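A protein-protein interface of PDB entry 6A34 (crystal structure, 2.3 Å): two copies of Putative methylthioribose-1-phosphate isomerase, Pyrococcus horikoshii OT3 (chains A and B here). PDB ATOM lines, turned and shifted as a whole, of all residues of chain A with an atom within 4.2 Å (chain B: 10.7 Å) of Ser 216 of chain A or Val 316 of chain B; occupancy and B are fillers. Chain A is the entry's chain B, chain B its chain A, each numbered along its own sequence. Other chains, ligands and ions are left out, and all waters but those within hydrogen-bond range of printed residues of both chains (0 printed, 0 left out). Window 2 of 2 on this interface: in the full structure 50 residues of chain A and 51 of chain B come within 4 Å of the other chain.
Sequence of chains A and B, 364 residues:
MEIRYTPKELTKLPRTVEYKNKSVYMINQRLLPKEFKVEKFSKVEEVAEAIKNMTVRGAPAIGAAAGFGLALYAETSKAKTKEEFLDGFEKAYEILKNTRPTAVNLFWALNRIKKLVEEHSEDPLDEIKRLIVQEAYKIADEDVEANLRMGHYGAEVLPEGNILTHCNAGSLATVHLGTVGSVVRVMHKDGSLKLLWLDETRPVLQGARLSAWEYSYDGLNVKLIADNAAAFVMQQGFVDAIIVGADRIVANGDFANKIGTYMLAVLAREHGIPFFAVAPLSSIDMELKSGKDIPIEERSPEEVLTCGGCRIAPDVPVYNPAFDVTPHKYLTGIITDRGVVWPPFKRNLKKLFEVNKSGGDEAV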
ATOM      1  N   ALA A 212       5.499  22.250 -15.698  1.00  0.00           N
ATOM      2  CA  ALA A 212       6.295  21.082 -15.413  1.00  0.00           C
ATOM      3  C   ALA A 212       7.573  21.522 -14.694  1.00  0.00           C
ATOM      4  O   ALA A 212       8.063  20.826 -13.791  1.00  0.00           O
ATOM      5  CB  ALA A 212       6.617  20.308 -16.675  1.00  0.00           C
ATOM      6  N   TRP A 213       8.110  22.675 -15.107  1.00  0.00           N
ATOM      7  CA  TRP A 213       9.340  23.194 -14.522  1.00  0.00           C
ATOM      8  C   TRP A 213       9.114  23.595 -13.054  1.00  0.00           C
ATOM      9  O   TRP A 213       9.852  23.145 -12.178  1.00  0.00           O
ATOM     10  CB  TRP A 213       9.952  24.339 -15.348  1.00  0.00           C
ATOM     11  CG  TRP A 213      11.241  24.788 -14.729  1.00  0.00           C
ATOM     12  CD1 TRP A 213      12.489  24.258 -14.908  1.00  0.00           C
ATOM     13  CD2 TRP A 213      11.377  25.818 -13.735  1.00  0.00           C
ATOM     14  NE1 TRP A 213      13.394  24.918 -14.125  1.00  0.00           N
ATOM     15  CE2 TRP A 213      12.745  25.876 -13.389  1.00  0.00           C
ATOM     16  CE3 TRP A 213      10.483  26.708 -13.138  1.00  0.00           C
ATOM     17  CZ2 TRP A 213      13.232  26.790 -12.450  1.00  0.00           C
ATOM     18  CZ3 TRP A 213      10.973  27.637 -12.238  1.00  0.00           C
ATOM     19  CH2 TRP A 213      12.325  27.675 -11.898  1.00  0.00           C
ATOM     20  N   GLU A 214       8.088  24.410 -12.774  1.00  0.00           N
ATOM     21  CA  GLU A 214       7.978  24.949 -11.423  1.00  0.00           C
ATOM     22  C   GLU A 214       7.501  23.878 -10.434  1.00  0.00           C
ATOM     23  O   GLU A 214       7.930  23.890  -9.275  1.00  0.00           O
ATOM     24  CB  GLU A 214       7.119  26.207 -11.374  1.00  0.00           C
ATOM     25  CG  GLU A 214       5.678  26.019 -11.799  1.00  0.00           C
ATOM     26  CD  GLU A 214       4.825  27.183 -11.351  1.00  0.00           C
ATOM     27  OE1 GLU A 214       4.451  27.198 -10.153  1.00  0.00           O
ATOM     28  OE2 GLU A 214       4.514  28.049 -12.206  1.00  0.00           O
ATOM     29  N   TYR A 215       6.604  22.969 -10.863  1.00  0.00           N
ATOM     30  CA  TYR A 215       6.050  21.980  -9.959  1.00  0.00           C
ATOM     31  C   TYR A 215       7.123  20.937  -9.631  1.00  0.00           C
ATOM     32  O   TYR A 215       7.252  20.491  -8.477  1.00  0.00           O
ATOM     33  CB  TYR A 215       4.759  21.377 -10.511  1.00  0.00           C
ATOM     34  CG  TYR A 215       3.612  22.347 -10.627  1.00  0.00           C
ATOM     35  CD1 TYR A 215       3.369  23.304  -9.659  1.00  0.00           C
ATOM     36  CD2 TYR A 215       2.766  22.318 -11.722  1.00  0.00           C
ATOM     37  CE1 TYR A 215       2.308  24.196  -9.779  1.00  0.00           C
ATOM     38  CE2 TYR A 215       1.703  23.199 -11.852  1.00  0.00           C
ATOM     39  CZ  TYR A 215       1.466  24.141 -10.874  1.00  0.00           C
ATOM     40  OH  TYR A 215       0.410  25.013 -11.015  1.00  0.00           O
ATOM     41  N   SER A 216       7.921  20.578 -10.632  1.00  0.00           N
ATOM     42  CA  SER A 216       9.052  19.719 -10.421  1.00  0.00           C
ATOM     43  C   SER A 216      10.092  20.385  -9.497  1.00  0.00           C
ATOM     44  O   SER A 216      10.660  19.706  -8.643  1.00  0.00           O
ATOM     45  CB  SER A 216       9.657  19.329 -11.716  1.00  0.00           C
ATOM     46  OG  SER A 216      10.795  18.508 -11.490  1.00  0.00           O
ATOM     47  N   TYR A 217      10.324  21.697  -9.646  1.00  0.00           N
ATOM     48  CA  TYR A 217      11.295  22.442  -8.777  1.00  0.00           C
ATOM     49  C   TYR A 217      10.943  22.267  -7.292  1.00  0.00           C
ATOM     50  O   TYR A 217      11.832  22.187  -6.428  1.00  0.00           O
ATOM     51  CB  TYR A 217      11.318  23.930  -9.123  1.00  0.00           C
ATOM     52  CG  TYR A 217      12.490  24.722  -8.588  1.00  0.00           C
ATOM     53  CD1 TYR A 217      13.682  24.799  -9.291  1.00  0.00           C
ATOM     54  CD2 TYR A 217      12.390  25.453  -7.412  1.00  0.00           C
ATOM     55  CE1 TYR A 217      14.749  25.559  -8.830  1.00  0.00           C
ATOM     56  CE2 TYR A 217      13.452  26.210  -6.930  1.00  0.00           C
ATOM     57  CZ  TYR A 217      14.636  26.268  -7.646  1.00  0.00           C
ATOM     58  OH  TYR A 217      15.681  27.020  -7.195  1.00  0.00           O
ATOM     59  N   ASP A 218       9.637  22.166  -7.025  1.00  0.00           N
ATOM     60  CA  ASP A 218       9.060  22.099  -5.687  1.00  0.00           C
ATOM     61  C   ASP A 218       8.829  20.650  -5.245  1.00  0.00           C
ATOM     62  O   ASP A 218       8.239  20.435  -4.219  1.00  0.00           O
ATOM     63  CB  ASP A 218       7.793  22.965  -5.606  1.00  0.00           C
ATOM     64  CG  ASP A 218       8.108  24.451  -5.452  1.00  0.00           C
ATOM     65  OD1 ASP A 218       9.226  24.735  -5.021  1.00  0.00           O
ATOM     66  OD2 ASP A 218       7.241  25.318  -5.768  1.00  0.00           O
ATOM     67  N   GLY A 219       9.328  19.671  -6.004  1.00  0.00           N
ATOM     68  CA  GLY A 219       9.270  18.257  -5.623  1.00  0.00           C
ATOM     69  C   GLY A 219       7.878  17.638  -5.729  1.00  0.00           C
ATOM     70  O   GLY A 219       7.668  16.570  -5.194  1.00  0.00           O
ATOM     71  N   LEU A 224       3.771  14.543 -17.255  1.00  0.00           N
ATOM     72  CA  LEU A 224       3.476  15.374 -18.405  1.00  0.00           C
ATOM     73  C   LEU A 224       2.876  14.486 -19.504  1.00  0.00           C
ATOM     74  O   LEU A 224       3.382  13.413 -19.745  1.00  0.00           O
ATOM     75  CB  LEU A 224       4.781  16.030 -18.856  1.00  0.00           C
ATOM     76  CG  LEU A 224       4.688  16.998 -20.029  1.00  0.00           C
ATOM     77  CD1 LEU A 224       3.904  18.263 -19.664  1.00  0.00           C
ATOM     78  CD2 LEU A 224       6.086  17.361 -20.510  1.00  0.00           C
ATOM     79  N   ARG B 299       5.186   4.680 -25.887  1.00  0.00           N
ATOM     80  CA  ARG B 299       6.410   4.926 -26.617  1.00  0.00           C
ATOM     81  C   ARG B 299       7.307   5.848 -25.791  1.00  0.00           C
ATOM     82  O   ARG B 299       6.949   6.229 -24.682  1.00  0.00           O
ATOM     83  CB  ARG B 299       6.091   5.471 -28.007  1.00  0.00           C
ATOM     84  CG  ARG B 299       5.391   4.430 -28.856  1.00  0.00           C
ATOM     85  CD  ARG B 299       5.150   4.868 -30.274  1.00  0.00           C
ATOM     86  NE  ARG B 299       4.715   3.667 -30.967  1.00  0.00           N
ATOM     87  CZ  ARG B 299       4.099   3.635 -32.143  1.00  0.00           C
ATOM     88  NH1 ARG B 299       3.684   2.466 -32.608  1.00  0.00           N
ATOM     89  NH2 ARG B 299       3.875   4.753 -32.824  1.00  0.00           N
ATOM     90  N   SER B 300       8.488   6.142 -26.349  1.00  0.00           N
ATOM     91  CA  SER B 300       9.537   6.812 -25.644  1.00  0.00           C
ATOM     92  C   SER B 300       9.023   8.130 -25.091  1.00  0.00           C
ATOM     93  O   SER B 300       8.294   8.871 -25.757  1.00  0.00           O
ATOM     94  CB  SER B 300      10.733   7.055 -26.523  1.00  0.00           C
ATOM     95  OG  SER B 300      11.566   8.055 -25.941  1.00  0.00           O
ATOM     96  N   PRO B 301       9.429   8.474 -23.858  1.00  0.00           N
ATOM     97  CA  PRO B 301       9.067   9.766 -23.284  1.00  0.00           C
ATOM     98  C   PRO B 301       9.632  10.956 -24.092  1.00  0.00           C
ATOM     99  O   PRO B 301       9.117  12.077 -24.012  1.00  0.00           O
ATOM    100  CB  PRO B 301       9.606   9.651 -21.847  1.00  0.00           C
ATOM    101  CG  PRO B 301      10.757   8.671 -21.957  1.00  0.00           C
ATOM    102  CD  PRO B 301      10.283   7.651 -22.982  1.00  0.00           C
ATOM    103  N   GLU B 302      10.635  10.705 -24.935  1.00  0.00           N
ATOM    104  CA  GLU B 302      11.241  11.760 -25.777  1.00  0.00           C
ATOM    105  C   GLU B 302      10.227  12.325 -26.778  1.00  0.00           C
ATOM    106  O   GLU B 302      10.324  13.493 -27.126  1.00  0.00           O
ATOM    107  CB  GLU B 302      12.481  11.247 -26.511  1.00  0.00           C
ATOM    108  CG  GLU B 302      13.636  10.908 -25.557  1.00  0.00           C
ATOM    109  CD  GLU B 302      14.236  12.083 -24.786  1.00  0.00           C
ATOM    110  OE1 GLU B 302      14.681  13.050 -25.432  1.00  0.00           O
ATOM    111  OE2 GLU B 302      14.292  12.012 -23.547  1.00  0.00           O
ATOM    112  N   GLU B 303       9.297  11.506 -27.272  1.00  0.00           N
ATOM    113  CA  GLU B 303       8.266  12.001 -28.162  1.00  0.00           C
ATOM    114  C   GLU B 303       7.452  13.140 -27.513  1.00  0.00           C
ATOM    115  O   GLU B 303       6.954  13.985 -28.221  1.00  0.00           O
ATOM    116  CB  GLU B 303       7.308  10.884 -28.566  1.00  0.00           C
ATOM    117  CG  GLU B 303       7.922   9.805 -29.434  1.00  0.00           C
ATOM    118  CD  GLU B 303       6.877   8.788 -29.900  1.00  0.00           C
ATOM    119  OE1 GLU B 303       5.772   8.742 -29.306  1.00  0.00           O
ATOM    120  OE2 GLU B 303       7.164   8.045 -30.853  1.00  0.00           O
ATOM    121  N   VAL B 304       7.341  13.170 -26.177  1.00  0.00           N
ATOM    122  CA  VAL B 304       6.597  14.261 -25.470  1.00  0.00           C
ATOM    123  C   VAL B 304       7.535  15.403 -25.007  1.00  0.00           C
ATOM    124  O   VAL B 304       7.112  16.571 -24.999  1.00  0.00           O
ATOM    125  CB  VAL B 304       5.782  13.690 -24.295  1.00  0.00           C
ATOM    126  CG1 VAL B 304       5.141  14.785 -23.463  1.00  0.00           C
ATOM    127  CG2 VAL B 304       4.722  12.692 -24.778  1.00  0.00           C
ATOM    128  N   LEU B 305       8.762  15.065 -24.579  1.00  0.00           N
ATOM    129  CA  LEU B 305       9.727  16.026 -24.033  1.00  0.00           C
ATOM    130  C   LEU B 305      10.250  16.905 -25.168  1.00  0.00           C
ATOM    131  O   LEU B 305      10.626  18.026 -24.907  1.00  0.00           O
ATOM    132  CB  LEU B 305      10.891  15.302 -23.344  1.00  0.00           C
ATOM    133  CG  LEU B 305      10.500  14.438 -22.152  1.00  0.00           C
ATOM    134  CD1 LEU B 305      11.682  13.632 -21.673  1.00  0.00           C
ATOM    135  CD2 LEU B 305       9.930  15.267 -21.014  1.00  0.00           C
ATOM    136  N   THR B 306      10.288  16.348 -26.389  1.00  0.00           N
ATOM    137  CA  THR B 306      10.610  17.073 -27.594  1.00  0.00           C
ATOM    138  C   THR B 306       9.374  17.212 -28.495  1.00  0.00           C
ATOM    139  O   THR B 306       8.395  16.461 -28.413  1.00  0.00           O
ATOM    140  CB  THR B 306      11.771  16.429 -28.362  1.00  0.00           C
ATOM    141  OG1 THR B 306      11.292  15.236 -28.975  1.00  0.00           O
ATOM    142  CG2 THR B 306      12.972  16.094 -27.502  1.00  0.00           C
ATOM    143  N   ARG B 311      13.629  20.643 -27.682  1.00  0.00           N
ATOM    144  CA  ARG B 311      13.333  20.144 -26.360  1.00  0.00           C
ATOM    145  C   ARG B 311      12.519  21.208 -25.628  1.00  0.00           C
ATOM    146  O   ARG B 311      12.992  22.284 -25.453  1.00  0.00           O
ATOM    147  CB  ARG B 311      14.618  19.814 -25.596  1.00  0.00           C
ATOM    148  CG  ARG B 311      14.348  19.250 -24.204  1.00  0.00           C
ATOM    149  CD  ARG B 311      15.507  18.491 -23.572  1.00  0.00           C
ATOM    150  NE  ARG B 311      15.977  17.393 -24.419  1.00  0.00           N
ATOM    151  CZ  ARG B 311      15.514  16.145 -24.410  1.00  0.00           C
ATOM    152  NH1 ARG B 311      14.692  15.723 -23.456  1.00  0.00           N
ATOM    153  NH2 ARG B 311      15.890  15.329 -25.379  1.00  0.00           N
ATOM    154  N   ILE B 312      11.296  20.881 -25.205  1.00  0.00           N
ATOM    155  CA  ILE B 312      10.334  21.896 -24.760  1.00  0.00           C
ATOM    156  C   ILE B 312       9.861  21.636 -23.321  1.00  0.00           C
ATOM    157  O   ILE B 312       8.927  22.296 -22.832  1.00  0.00           O
ATOM    158  CB  ILE B 312       9.155  22.015 -25.756  1.00  0.00           C
ATOM    159  CG1 ILE B 312       8.531  20.671 -26.152  1.00  0.00           C
ATOM    160  CG2 ILE B 312       9.591  22.785 -27.008  1.00  0.00           C
ATOM    161  CD1 ILE B 312       7.674  19.986 -25.082  1.00  0.00           C
ATOM    162  N   ALA B 313      10.471  20.671 -22.641  1.00  0.00           N
ATOM    163  CA  ALA B 313      10.096  20.301 -21.290  1.00  0.00           C
ATOM    164  C   ALA B 313      11.366  19.988 -20.527  1.00  0.00           C
ATOM    165  O   ALA B 313      12.323  19.507 -21.125  1.00  0.00           O
ATOM    166  CB  ALA B 313       9.191  19.088 -21.271  1.00  0.00           C
ATOM    167  N   PRO B 314      11.352  20.159 -19.190  1.00  0.00           N
ATOM    168  CA  PRO B 314      12.443  19.695 -18.333  1.00  0.00           C
ATOM    169  C   PRO B 314      12.387  18.175 -18.187  1.00  0.00           C
ATOM    170  O   PRO B 314      11.416  17.542 -18.634  1.00  0.00           O
ATOM    171  CB  PRO B 314      12.145  20.363 -16.983  1.00  0.00           C
ATOM    172  CG  PRO B 314      10.659  20.597 -16.981  1.00  0.00           C
ATOM    173  CD  PRO B 314      10.225  20.708 -18.426  1.00  0.00           C
ATOM    174  N   ASP B 315      13.396  17.603 -17.540  1.00  0.00           N
ATOM    175  CA  ASP B 315      13.458  16.169 -17.328  1.00  0.00           C
ATOM    176  C   ASP B 315      12.430  15.812 -16.251  1.00  0.00           C
ATOM    177  O   ASP B 315      12.682  15.955 -15.059  1.00  0.00           O
ATOM    178  CB  ASP B 315      14.873  15.708 -16.948  1.00  0.00           C
ATOM    179  CG  ASP B 315      14.986  14.254 -16.484  1.00  0.00           C
ATOM    180  OD1 ASP B 315      14.005  13.486 -16.648  1.00  0.00           O
ATOM    181  OD2 ASP B 315      16.069  13.888 -15.962  1.00  0.00           O
ATOM    182  N   VAL B 316      11.247  15.392 -16.698  1.00  0.00           N
ATOM    183  CA  VAL B 316      10.178  15.058 -15.822  1.00  0.00           C
ATOM    184  C   VAL B 316       9.566  13.764 -16.338  1.00  0.00           C
ATOM    185  O   VAL B 316       9.691  13.436 -17.507  1.00  0.00           O
ATOM    186  CB  VAL B 316       9.126  16.187 -15.714  1.00  0.00           C
ATOM    187  CG1 VAL B 316       9.704  17.442 -15.080  1.00  0.00           C
ATOM    188  CG2 VAL B 316       8.468  16.506 -17.050  1.00  0.00           C
ATOM    189  N   PRO B 317       8.864  12.997 -15.490  1.00  0.00           N
ATOM    190  CA  PRO B 317       8.195  11.784 -15.958  1.00  0.00           C
ATOM    191  C   PRO B 317       7.095  12.125 -16.986  1.00  0.00           C
ATOM    192  O   PRO B 317       6.463  13.145 -16.888  1.00  0.00           O
ATOM    193  CB  PRO B 317       7.610  11.167 -14.673  1.00  0.00           C
ATOM    194  CG  PRO B 317       8.313  11.883 -13.508  1.00  0.00           C
ATOM    195  CD  PRO B 317       8.695  13.247 -14.045  1.00  0.00           C
ATOM    196  N   VAL B 318       6.898  11.247 -17.965  1.00  0.00           N
ATOM    197  CA  VAL B 318       5.945  11.397 -19.028  1.00  0.00           C
ATOM    198  C   VAL B 318       5.071  10.141 -19.075  1.00  0.00           C
ATOM    199  O   VAL B 318       5.516   9.065 -18.720  1.00  0.00           O
ATOM    200  CB  VAL B 318       6.697  11.547 -20.363  1.00  0.00           C
ATOM    201  CG1 VAL B 318       5.803  11.277 -21.563  1.00  0.00           C
ATOM    202  CG2 VAL B 318       7.371  12.900 -20.465  1.00  0.00           C
ATOM    203  N   TYR B 319       3.863  10.275 -19.615  1.00  0.00           N
ATOM    204  CA  TYR B 319       3.097   9.123 -20.023  1.00  0.00           C
ATOM    205  C   TYR B 319       2.721   9.313 -21.488  1.00  0.00           C
ATOM    206  O   TYR B 319       2.130  10.314 -21.833  1.00  0.00           O
ATOM    207  CB  TYR B 319       1.874   8.974 -19.129  1.00  0.00           C
ATOM    208  CG  TYR B 319       1.015   7.777 -19.428  1.00  0.00           C
ATOM    209  CD1 TYR B 319       1.542   6.495 -19.437  1.00  0.00           C
ATOM    210  CD2 TYR B 319      -0.332   7.931 -19.665  1.00  0.00           C
ATOM    211  CE1 TYR B 319       0.737   5.391 -19.693  1.00  0.00           C
ATOM    212  CE2 TYR B 319      -1.144   6.845 -19.937  1.00  0.00           C
ATOM    213  CZ  TYR B 319      -0.612   5.570 -19.927  1.00  0.00           C
ATOM    214  OH  TYR B 319      -1.436   4.525 -20.179  1.00  0.00           O
ATOM    215  N   ASN B 320       3.147   8.375 -22.330  1.00  0.00           N
ATOM    216  CA  ASN B 320       3.025   8.506 -23.751  1.00  0.00           C
ATOM    217  C   ASN B 320       2.310   7.288 -24.348  1.00  0.00           C
ATOM    218  O   ASN B 320       2.896   6.517 -25.101  1.00  0.00           O
ATOM    219  CB  ASN B 320       4.391   8.685 -24.411  1.00  0.00           C
ATOM    220  CG  ASN B 320       4.238   8.940 -25.896  1.00  0.00           C
ATOM    221  OD1 ASN B 320       3.162   9.318 -26.328  1.00  0.00           O
ATOM    222  ND2 ASN B 320       5.293   8.755 -26.672  1.00  0.00           N
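Hydrophobic or aromatic side chains of chain A that line the printed part of chain B: Leu 224. Printed residues of chain B that touch a printed residue of chain A: Ala 313, Pro 314, Val 316, Pro 317, Val 318 and Tyr 319. Along chain B the printed residues that touch a printed residue of chain A span positions 313 to 319. Among the printed residues, 8 pairs touch across the chains. Among the printed residues, no Asp or Glu carboxylate lies within 4 Å of a Lys or Arg side-chain nitrogen of the other chain.
N of Leu 224 of chain A is in hydrogen-bond range of O of Pro 317 of chain B (3.1 Å). O of Leu 224 of chain A is in hydrogen-bond range of N of Tyr 319 of chain B, 3.2 Å away.
Of chain B, only Pro 314 (3.95 Å) and Val 316 (3.98 Å) come within 4 Å of Ala 212 of chain A. Glu 214 of chain A touches none of the printed residues of chain B. No residue of chain B comes within 4 Å of Gly 219 of chain A. Glu 302 of chain B touches none of the printed residues of chain A. Val 316 of chain B touches just these residues of chain A: Ala 212 and Ser 216. Of the printed residues of chain A, Pro 317 of chain B touches Leu 224 (3.1 Å). Printed residues of chain A within 4 Å of Tyr 319 of chain B: Leu 224. The nearest residue of chain B that does not touch Ser 216 of chain A is Asp 315 of chain B (4.8 Å). The nearest printed residue of chain B that does not touch Trp 213 of chain A is Val 316 of chain B (5.5 Å).
The backbone carbonyl oxygen (O) of Leu 305 of chain B is in hydrogen-bond range of the backbone NH (N) of Ala 313 of chain B (3.5 Å).
No position is printed for both chains.
Pro 314 of chain B touches Ala 212 of chain A (CG to C, 3.95 Å). Ala 212 of chain A touches Val 316 of chain B. Pro 314 of chain B touches Trp 213 of chain A. Val 316 of chain B touches Ser 216 of chain A. Ala 313 of chain B touches Leu 224 of chain A (CB to CD2, 3.6 Å). Leu 224 of chain A touches Val 318 of chain B.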
